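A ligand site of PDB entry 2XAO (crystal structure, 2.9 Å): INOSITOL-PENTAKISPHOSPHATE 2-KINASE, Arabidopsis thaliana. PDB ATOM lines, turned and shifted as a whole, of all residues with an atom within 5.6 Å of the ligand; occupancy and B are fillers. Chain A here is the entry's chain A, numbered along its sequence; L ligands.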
ATOM      1  N   GLU A  18     -16.765 -12.260  -7.380  1.00  0.00           N
ATOM      2  CA  GLU A  18     -16.453 -10.891  -6.939  1.00  0.00           C
ATOM      3  C   GLU A  18     -15.307 -10.771  -5.912  1.00  0.00           C
ATOM      4  O   GLU A  18     -15.044 -11.703  -5.132  1.00  0.00           O
ATOM      5  CB  GLU A  18     -17.700 -10.253  -6.337  1.00  0.00           C
ATOM      6  CG  GLU A  18     -18.136 -10.904  -5.046  1.00  0.00           C
ATOM      7  CD  GLU A  18     -19.572 -10.662  -4.754  1.00  0.00           C
ATOM      8  OE1 GLU A  18     -20.383 -11.554  -5.076  1.00  0.00           O
ATOM      9  OE2 GLU A  18     -19.893  -9.566  -4.235  1.00  0.00           O
ATOM     10  N   GLY A  19     -14.658  -9.610  -5.911  1.00  0.00           N
ATOM     11  CA  GLY A  19     -13.748  -9.233  -4.837  1.00  0.00           C
ATOM     12  C   GLY A  19     -14.412  -8.307  -3.828  1.00  0.00           C
ATOM     13  O   GLY A  19     -15.646  -8.284  -3.692  1.00  0.00           O
ATOM     14  N   GLY A  20     -13.601  -7.553  -3.092  1.00  0.00           N
ATOM     15  CA  GLY A  20     -14.127  -6.565  -2.175  1.00  0.00           C
ATOM     16  C   GLY A  20     -14.729  -5.401  -2.946  1.00  0.00           C
ATOM     17  O   GLY A  20     -15.814  -4.920  -2.607  1.00  0.00           O
ATOM     18  N   ALA A  21     -14.023  -4.966  -3.992  1.00  0.00           N
ATOM     19  CA  ALA A  21     -14.387  -3.765  -4.772  1.00  0.00           C
ATOM     20  C   ALA A  21     -15.365  -3.999  -5.944  1.00  0.00           C
ATOM     21  O   ALA A  21     -16.208  -3.133  -6.254  1.00  0.00           O
ATOM     22  CB  ALA A  21     -13.100  -3.087  -5.283  1.00  0.00           C
ATOM     23  N   ARG A  45     -20.222   0.444  -1.533  1.00  0.00           N
ATOM     24  CA  ARG A  45     -19.992  -0.008  -0.171  1.00  0.00           C
ATOM     25  C   ARG A  45     -20.919   0.739   0.803  1.00  0.00           C
ATOM     26  O   ARG A  45     -20.890   1.968   0.870  1.00  0.00           O
ATOM     27  CB  ARG A  45     -18.514   0.180   0.200  1.00  0.00           C
ATOM     28  CG  ARG A  45     -17.574  -0.472  -0.804  1.00  0.00           C
ATOM     29  CD  ARG A  45     -16.111  -0.261  -0.453  1.00  0.00           C
ATOM     30  NE  ARG A  45     -15.210  -1.185  -1.158  1.00  0.00           N
ATOM     31  CZ  ARG A  45     -14.585  -2.218  -0.585  1.00  0.00           C
ATOM     32  NH1 ARG A  45     -14.753  -2.492   0.702  1.00  0.00           N
ATOM     33  NH2 ARG A  45     -13.773  -2.994  -1.300  1.00  0.00           N
ATOM     34  N   TRP A 129     -23.419 -12.752   2.826  1.00  0.00           N
ATOM     35  CA  TRP A 129     -22.569 -11.761   3.486  1.00  0.00           C
ATOM     36  C   TRP A 129     -22.017 -10.705   2.508  1.00  0.00           C
ATOM     37  O   TRP A 129     -21.772  -9.557   2.883  1.00  0.00           O
ATOM     38  CB  TRP A 129     -21.444 -12.434   4.295  1.00  0.00           C
ATOM     39  CG  TRP A 129     -20.286 -12.991   3.472  1.00  0.00           C
ATOM     40  CD1 TRP A 129     -20.182 -14.245   2.947  1.00  0.00           C
ATOM     41  CD2 TRP A 129     -19.073 -12.303   3.111  1.00  0.00           C
ATOM     42  NE1 TRP A 129     -18.983 -14.388   2.282  1.00  0.00           N
ATOM     43  CE2 TRP A 129     -18.284 -13.211   2.355  1.00  0.00           C
ATOM     44  CE3 TRP A 129     -18.575 -11.013   3.326  1.00  0.00           C
ATOM     45  CZ2 TRP A 129     -17.039 -12.869   1.833  1.00  0.00           C
ATOM     46  CZ3 TRP A 129     -17.339 -10.670   2.807  1.00  0.00           C
ATOM     47  CH2 TRP A 129     -16.578 -11.600   2.073  1.00  0.00           C
ATOM     48  N   ARG A 130     -21.805 -11.102   1.253  1.00  0.00           N
ATOM     49  CA  ARG A 130     -21.339 -10.159   0.229  1.00  0.00           C
ATOM     50  C   ARG A 130     -22.457  -9.198  -0.106  1.00  0.00           C
ATOM     51  O   ARG A 130     -22.227  -7.992  -0.187  1.00  0.00           O
ATOM     52  CB  ARG A 130     -20.843 -10.886  -1.028  1.00  0.00           C
ATOM     53  CG  ARG A 130     -19.485 -11.596  -0.903  1.00  0.00           C
ATOM     54  CD  ARG A 130     -18.315 -10.623  -1.047  1.00  0.00           C
ATOM     55  NE  ARG A 130     -17.108 -11.277  -1.576  1.00  0.00           N
ATOM     56  CZ  ARG A 130     -15.857 -10.886  -1.321  1.00  0.00           C
ATOM     57  NH1 ARG A 130     -15.612  -9.863  -0.537  1.00  0.00           N
ATOM     58  NH2 ARG A 130     -14.848 -11.548  -1.830  1.00  0.00           N
ATOM     59  N   LYS A 168      -4.669 -16.263  -5.666  1.00  0.00           N
ATOM     60  CA  LYS A 168      -4.470 -14.990  -4.962  1.00  0.00           C
ATOM     61  C   LYS A 168      -3.351 -15.176  -3.915  1.00  0.00           C
ATOM     62  O   LYS A 168      -3.644 -15.557  -2.785  1.00  0.00           O
ATOM     63  CB  LYS A 168      -5.780 -14.565  -4.299  1.00  0.00           C
ATOM     64  CG  LYS A 168      -5.730 -13.335  -3.424  1.00  0.00           C
ATOM     65  CD  LYS A 168      -7.152 -12.946  -3.004  1.00  0.00           C
ATOM     66  CE  LYS A 168      -7.188 -11.981  -1.812  1.00  0.00           C
ATOM     67  NZ  LYS A 168      -7.716 -10.641  -2.120  1.00  0.00           N
ATOM     68  N   LYS A 170      -1.279 -13.330  -2.042  1.00  0.00           N
ATOM     69  CA  LYS A 170      -1.061 -12.457  -0.852  1.00  0.00           C
ATOM     70  C   LYS A 170       0.420 -12.145  -0.642  1.00  0.00           C
ATOM     71  O   LYS A 170       1.204 -12.225  -1.565  1.00  0.00           O
ATOM     72  CB  LYS A 170      -1.701 -13.028   0.432  1.00  0.00           C
ATOM     73  CG  LYS A 170      -3.196 -13.240   0.384  1.00  0.00           C
ATOM     74  CD  LYS A 170      -3.996 -11.965   0.093  1.00  0.00           C
ATOM     75  CE  LYS A 170      -4.056 -11.015   1.252  1.00  0.00           C
ATOM     76  NZ  LYS A 170      -5.229 -10.108   1.203  1.00  0.00           N
ATOM     77  N   ARG A 192       2.273 -12.674   7.594  1.00  0.00           N
ATOM     78  CA  ARG A 192       1.033 -11.959   7.855  1.00  0.00           C
ATOM     79  C   ARG A 192      -0.197 -12.846   7.591  1.00  0.00           C
ATOM     80  O   ARG A 192      -1.121 -12.876   8.404  1.00  0.00           O
ATOM     81  CB  ARG A 192       1.002 -10.686   7.020  1.00  0.00           C
ATOM     82  CG  ARG A 192      -0.352 -10.111   6.778  1.00  0.00           C
ATOM     83  CD  ARG A 192      -0.879  -9.352   7.967  1.00  0.00           C
ATOM     84  NE  ARG A 192      -1.859  -8.395   7.477  1.00  0.00           N
ATOM     85  CZ  ARG A 192      -1.788  -7.075   7.628  1.00  0.00           C
ATOM     86  NH1 ARG A 192      -0.790  -6.501   8.298  1.00  0.00           N
ATOM     87  NH2 ARG A 192      -2.753  -6.334   7.118  1.00  0.00           N
ATOM     88  N   HIS A 196      -3.183 -13.559  10.284  1.00  0.00           N
ATOM     89  CA  HIS A 196      -4.539 -13.188   9.942  1.00  0.00           C
ATOM     90  C   HIS A 196      -5.505 -14.382   9.997  1.00  0.00           C
ATOM     91  O   HIS A 196      -6.659 -14.246  10.431  1.00  0.00           O
ATOM     92  CB  HIS A 196      -4.547 -12.558   8.558  1.00  0.00           C
ATOM     93  CG  HIS A 196      -5.622 -11.545   8.381  1.00  0.00           C
ATOM     94  ND1 HIS A 196      -5.587 -10.603   7.381  1.00  0.00           N
ATOM     95  CD2 HIS A 196      -6.751 -11.315   9.086  1.00  0.00           C
ATOM     96  CE1 HIS A 196      -6.658  -9.838   7.466  1.00  0.00           C
ATOM     97  NE2 HIS A 196      -7.376 -10.243   8.496  1.00  0.00           N
ATOM     98  N   LYS A 200      -9.171 -14.316  11.615  1.00  0.00           N
ATOM     99  CA  LYS A 200     -10.303 -14.714  10.768  1.00  0.00           C
ATOM    100  C   LYS A 200     -11.128 -15.860  11.379  1.00  0.00           C
ATOM    101  O   LYS A 200     -12.350 -15.830  11.334  1.00  0.00           O
ATOM    102  CB  LYS A 200      -9.814 -15.069   9.371  1.00  0.00           C
ATOM    103  CG  LYS A 200      -9.386 -13.850   8.580  1.00  0.00           C
ATOM    104  CD  LYS A 200      -8.581 -14.221   7.355  1.00  0.00           C
ATOM    105  CE  LYS A 200      -8.371 -13.018   6.440  1.00  0.00           C
ATOM    106  NZ  LYS A 200      -8.937 -13.238   5.097  1.00  0.00           N
ATOM    107  N   ASN A 238     -10.138 -18.249  -0.322  1.00  0.00           N
ATOM    108  CA  ASN A 238     -10.330 -17.299  -1.421  1.00  0.00           C
ATOM    109  C   ASN A 238      -9.064 -17.132  -2.264  1.00  0.00           C
ATOM    110  O   ASN A 238      -8.888 -16.120  -2.957  1.00  0.00           O
ATOM    111  CB  ASN A 238     -10.886 -15.948  -0.913  1.00  0.00           C
ATOM    112  CG  ASN A 238      -9.894 -15.158  -0.044  1.00  0.00           C
ATOM    113  OD1 ASN A 238     -10.177 -14.018   0.324  1.00  0.00           O
ATOM    114  ND2 ASN A 238      -8.745 -15.730   0.282  1.00  0.00           N
ATOM    115  N   ALA A 364       0.514  -2.500  -1.585  1.00  0.00           N
ATOM    116  CA  ALA A 364      -0.800  -2.983  -1.229  1.00  0.00           C
ATOM    117  C   ALA A 364      -1.554  -3.520  -2.463  1.00  0.00           C
ATOM    118  O   ALA A 364      -2.240  -4.534  -2.356  1.00  0.00           O
ATOM    119  CB  ALA A 364      -1.587  -1.898  -0.509  1.00  0.00           C
ATOM    120  N   ASP A 368      -2.556  -7.788  -2.921  1.00  0.00           N
ATOM    121  CA  ASP A 368      -3.955  -8.197  -2.982  1.00  0.00           C
ATOM    122  C   ASP A 368      -4.450  -8.486  -4.400  1.00  0.00           C
ATOM    123  O   ASP A 368      -5.648  -8.520  -4.650  1.00  0.00           O
ATOM    124  CB  ASP A 368      -4.838  -7.145  -2.340  1.00  0.00           C
ATOM    125  CG  ASP A 368      -6.223  -7.662  -1.989  1.00  0.00           C
ATOM    126  OD1 ASP A 368      -6.303  -8.613  -1.172  1.00  0.00           O
ATOM    127  OD2 ASP A 368      -7.225  -7.123  -2.520  1.00  0.00           O
ATOM    128  N   SER A 409      -6.272  -3.345  -7.783  1.00  0.00           N
ATOM    129  CA  SER A 409      -6.974  -2.135  -7.384  1.00  0.00           C
ATOM    130  C   SER A 409      -6.077  -1.023  -6.821  1.00  0.00           C
ATOM    131  O   SER A 409      -5.074  -1.280  -6.132  1.00  0.00           O
ATOM    132  CB  SER A 409      -8.083  -2.461  -6.398  1.00  0.00           C
ATOM    133  OG  SER A 409      -8.902  -3.497  -6.893  1.00  0.00           O
ATOM    134  N   LEU A 410      -6.448   0.219  -7.129  1.00  0.00           N
ATOM    135  CA  LEU A 410      -5.901   1.360  -6.416  1.00  0.00           C
ATOM    136  C   LEU A 410      -6.406   1.292  -4.985  1.00  0.00           C
ATOM    137  O   LEU A 410      -7.553   0.927  -4.750  1.00  0.00           O
ATOM    138  CB  LEU A 410      -6.336   2.671  -7.081  1.00  0.00           C
ATOM    139  CG  LEU A 410      -6.237   3.955  -6.241  1.00  0.00           C
ATOM    140  CD1 LEU A 410      -4.807   4.370  -6.006  1.00  0.00           C
ATOM    141  CD2 LEU A 410      -7.031   5.077  -6.872  1.00  0.00           C
ATOM    142  N   LYS A 411      -5.563   1.628  -4.023  1.00  0.00           N
ATOM    143  CA  LYS A 411      -5.966   1.608  -2.623  1.00  0.00           C
ATOM    144  C   LYS A 411      -6.161   3.027  -2.090  1.00  0.00           C
ATOM    145  O   LYS A 411      -5.277   3.870  -2.207  1.00  0.00           O
ATOM    146  CB  LYS A 411      -4.946   0.813  -1.791  1.00  0.00           C
ATOM    147  CG  LYS A 411      -4.709  -0.619  -2.319  1.00  0.00           C
ATOM    148  CD  LYS A 411      -5.973  -1.489  -2.238  1.00  0.00           C
ATOM    149  CE  LYS A 411      -5.766  -2.875  -2.873  1.00  0.00           C
ATOM    150  NZ  LYS A 411      -6.757  -3.899  -2.385  1.00  0.00           N
ATOM    151  N   ARG A 415      -7.059   4.533   3.903  1.00  0.00           N
ATOM    152  CA  ARG A 415      -6.878   3.196   4.496  1.00  0.00           C
ATOM    153  C   ARG A 415      -5.574   3.037   5.297  1.00  0.00           C
ATOM    154  O   ARG A 415      -5.439   2.080   6.059  1.00  0.00           O
ATOM    155  CB  ARG A 415      -6.948   2.136   3.407  1.00  0.00           C
ATOM    156  CG  ARG A 415      -7.746   0.947   3.810  1.00  0.00           C
ATOM    157  CD  ARG A 415      -7.984   0.026   2.616  1.00  0.00           C
ATOM    158  NE  ARG A 415      -9.175   0.362   1.848  1.00  0.00           N
ATOM    159  CZ  ARG A 415      -9.580  -0.356   0.793  1.00  0.00           C
ATOM    160  NH1 ARG A 415      -8.897  -1.436   0.412  1.00  0.00           N
ATOM    161  NH2 ARG A 415     -10.679  -0.018   0.134  1.00  0.00           N
ATOM    162  N   TYR A 419      -5.100   0.309   7.987  1.00  0.00           N
ATOM    163  CA  TYR A 419      -4.061  -0.716   7.887  1.00  0.00           C
ATOM    164  C   TYR A 419      -3.356  -0.902   9.215  1.00  0.00           C
ATOM    165  O   TYR A 419      -3.245  -2.029   9.706  1.00  0.00           O
ATOM    166  CB  TYR A 419      -3.032  -0.425   6.784  1.00  0.00           C
ATOM    167  CG  TYR A 419      -3.564  -0.606   5.368  1.00  0.00           C
ATOM    168  CD1 TYR A 419      -3.102   0.200   4.330  1.00  0.00           C
ATOM    169  CD2 TYR A 419      -4.531  -1.584   5.066  1.00  0.00           C
ATOM    170  CE1 TYR A 419      -3.591   0.044   3.026  1.00  0.00           C
ATOM    171  CE2 TYR A 419      -5.017  -1.743   3.771  1.00  0.00           C
ATOM    172  CZ  TYR A 419      -4.539  -0.922   2.769  1.00  0.00           C
ATOM    173  OH  TYR A 419      -5.009  -1.069   1.485  1.00  0.00           O
ATOM    174  N   LEU A 422      -5.641  -2.616  11.874  1.00  0.00           N
ATOM    175  CA  LEU A 422      -5.842  -4.035  11.582  1.00  0.00           C
ATOM    176  C   LEU A 422      -4.581  -4.828  11.858  1.00  0.00           C
ATOM    177  O   LEU A 422      -4.621  -5.906  12.449  1.00  0.00           O
ATOM    178  CB  LEU A 422      -6.267  -4.213  10.136  1.00  0.00           C
ATOM    179  CG  LEU A 422      -6.279  -5.600   9.520  1.00  0.00           C
ATOM    180  CD1 LEU A 422      -7.229  -6.504  10.252  1.00  0.00           C
ATOM    181  CD2 LEU A 422      -6.648  -5.504   8.031  1.00  0.00           C
HETATM  182  O1  LIG L   1     -12.533 -11.169  -0.423  1.00  0.00           O
HETATM  183  P1  LIG L   1     -12.103 -10.282   0.722  1.00  0.00           P
HETATM  184  O2  LIG L   1     -12.902  -9.016   0.947  1.00  0.00           O
HETATM  185  O3  LIG L   1     -11.752 -11.047   1.979  1.00  0.00           O
HETATM  186  O4  LIG L   1     -10.714  -9.695   0.174  1.00  0.00           O
HETATM  187  C1  LIG L   1     -10.208  -8.504   0.751  1.00  0.00           C
HETATM  188  C2  LIG L   1     -10.171  -7.427  -0.326  1.00  0.00           C
HETATM  189  O5  LIG L   1      -9.530  -7.947  -1.501  1.00  0.00           O
HETATM  190  C3  LIG L   1      -9.487  -6.160   0.209  1.00  0.00           C
HETATM  191  O6  LIG L   1      -9.259  -5.215  -0.823  1.00  0.00           O
HETATM  192  P2  LIG L   1     -10.450  -4.338  -1.478  1.00  0.00           P
HETATM  193  O7  LIG L   1      -9.672  -3.212  -2.152  1.00  0.00           O
HETATM  194  O8  LIG L   1     -11.335  -3.885  -0.329  1.00  0.00           O
HETATM  195  O9  LIG L   1     -11.160  -5.301  -2.416  1.00  0.00           O
HETATM  196  C4  LIG L   1      -8.845  -8.808   1.358  1.00  0.00           C
HETATM  197  O10 LIG L   1      -8.949  -9.707   2.476  1.00  0.00           O
HETATM  198  P3  LIG L   1      -8.203 -11.136   2.500  1.00  0.00           P
HETATM  199  O11 LIG L   1      -7.497 -11.280   1.177  1.00  0.00           O
HETATM  200  O12 LIG L   1      -9.319 -12.125   2.712  1.00  0.00           O
HETATM  201  O13 LIG L   1      -7.260 -11.001   3.673  1.00  0.00           O
HETATM  202  C5  LIG L   1      -8.184  -7.556   1.894  1.00  0.00           C
HETATM  203  O14 LIG L   1      -6.864  -7.977   2.157  1.00  0.00           O
HETATM  204  P4  LIG L   1      -6.183  -7.868   3.599  1.00  0.00           P
HETATM  205  O15 LIG L   1      -7.012  -8.760   4.515  1.00  0.00           O
HETATM  206  O16 LIG L   1      -6.270  -6.408   3.937  1.00  0.00           O
HETATM  207  O17 LIG L   1      -4.789  -8.368   3.263  1.00  0.00           O
HETATM  208  C6  LIG L   1      -8.133  -6.434   0.867  1.00  0.00           C
HETATM  209  O18 LIG L   1      -7.768  -5.248   1.562  1.00  0.00           O
HETATM  210  P5  LIG L   1      -6.412  -4.454   1.318  1.00  0.00           P
HETATM  211  O19 LIG L   1      -5.538  -4.821   2.472  1.00  0.00           O
HETATM  212  O20 LIG L   1      -5.884  -4.959   0.002  1.00  0.00           O
HETATM  213  O21 LIG L   1      -6.884  -3.018   1.341  1.00  0.00           O
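NZ of Lys 170 lies within salt-bridge range of O11 of the ligand. The side-chain carboxylate of Asp 368 is in hydrogen-bond range of an oxygen (O5) of the ligand, at 2.7 Å. The side-chain amino group of Lys 200 is in salt-bridge range of an oxygen (O12) of the ligand, 2.7 Å away. An oxygen (O21) of the ligand sits at hydrogen-bond distance from the side-chain hydroxyl (OH) of Tyr 419. The guanidinium group of Arg 415 is in salt-bridge range of an oxygen (O21) of the ligand, 2.7 Å away. NH2 of Arg 130 lies within salt-bridge range of O1 of the ligand (2.7 Å). The side-chain amino group (NZ) of Lys 411 lies within salt-bridge range of an oxygen (O20) of the ligand (2.8 Å). The guanidinium group of Arg 45 is in salt-bridge range of an oxygen (O8) of the ligand (2.8 Å). An oxygen (O11) of the ligand is in salt-bridge range of the side-chain amino group (NZ) of Lys 168. An oxygen (O12) of the ligand sits close to the side-chain amide oxygen (OD1) of Asn 238, at 3.2 Å. An oxygen (O9) of the ligand sits close to the backbone NH (N) of Gly 20 (3.4 Å). N of Ala 21 is in hydrogen-bond range of O9 of the ligand, at 3.3 Å.
The side-chain amino group of Lys 170 is in salt-bridge range of the side-chain carboxylate of Asp 368 (3.0 Å). OD2 of Asp 368 lies within salt-bridge range of NZ of Lys 411, at 3.3 Å. The side-chain carboxylate (OD1) of Asp 368 lies within salt-bridge range of the side-chain amino group (NZ) of Lys 168, 2.6 Å away. The backbone carbonyl oxygen (O) of Glu 18 sits at hydrogen-bond distance from the guanidinium group (NH2) of Arg 130 (3.3 Å). The guanidinium group (NH2) of Arg 45 sits close to the backbone carbonyl oxygen (O) of Gly 20, 3.1 Å away.
His 196 touches the ligand (CE1 to O15, 3.2 Å). Hydrophobic or aromatic side chains within 4 Å of the ligand: His 196 and Tyr 419. 13 residues have an atom within 4 Å of the ligand: Gly 20, Ala 21, Arg 45, Arg 130, Lys 168, Lys 170, His 196, Lys 200, Asn 238, Asp 368, Lys 411, Arg 415 and Tyr 419. The nearest printed residue that does not touch the ligand is Leu 422 (4.2 Å).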
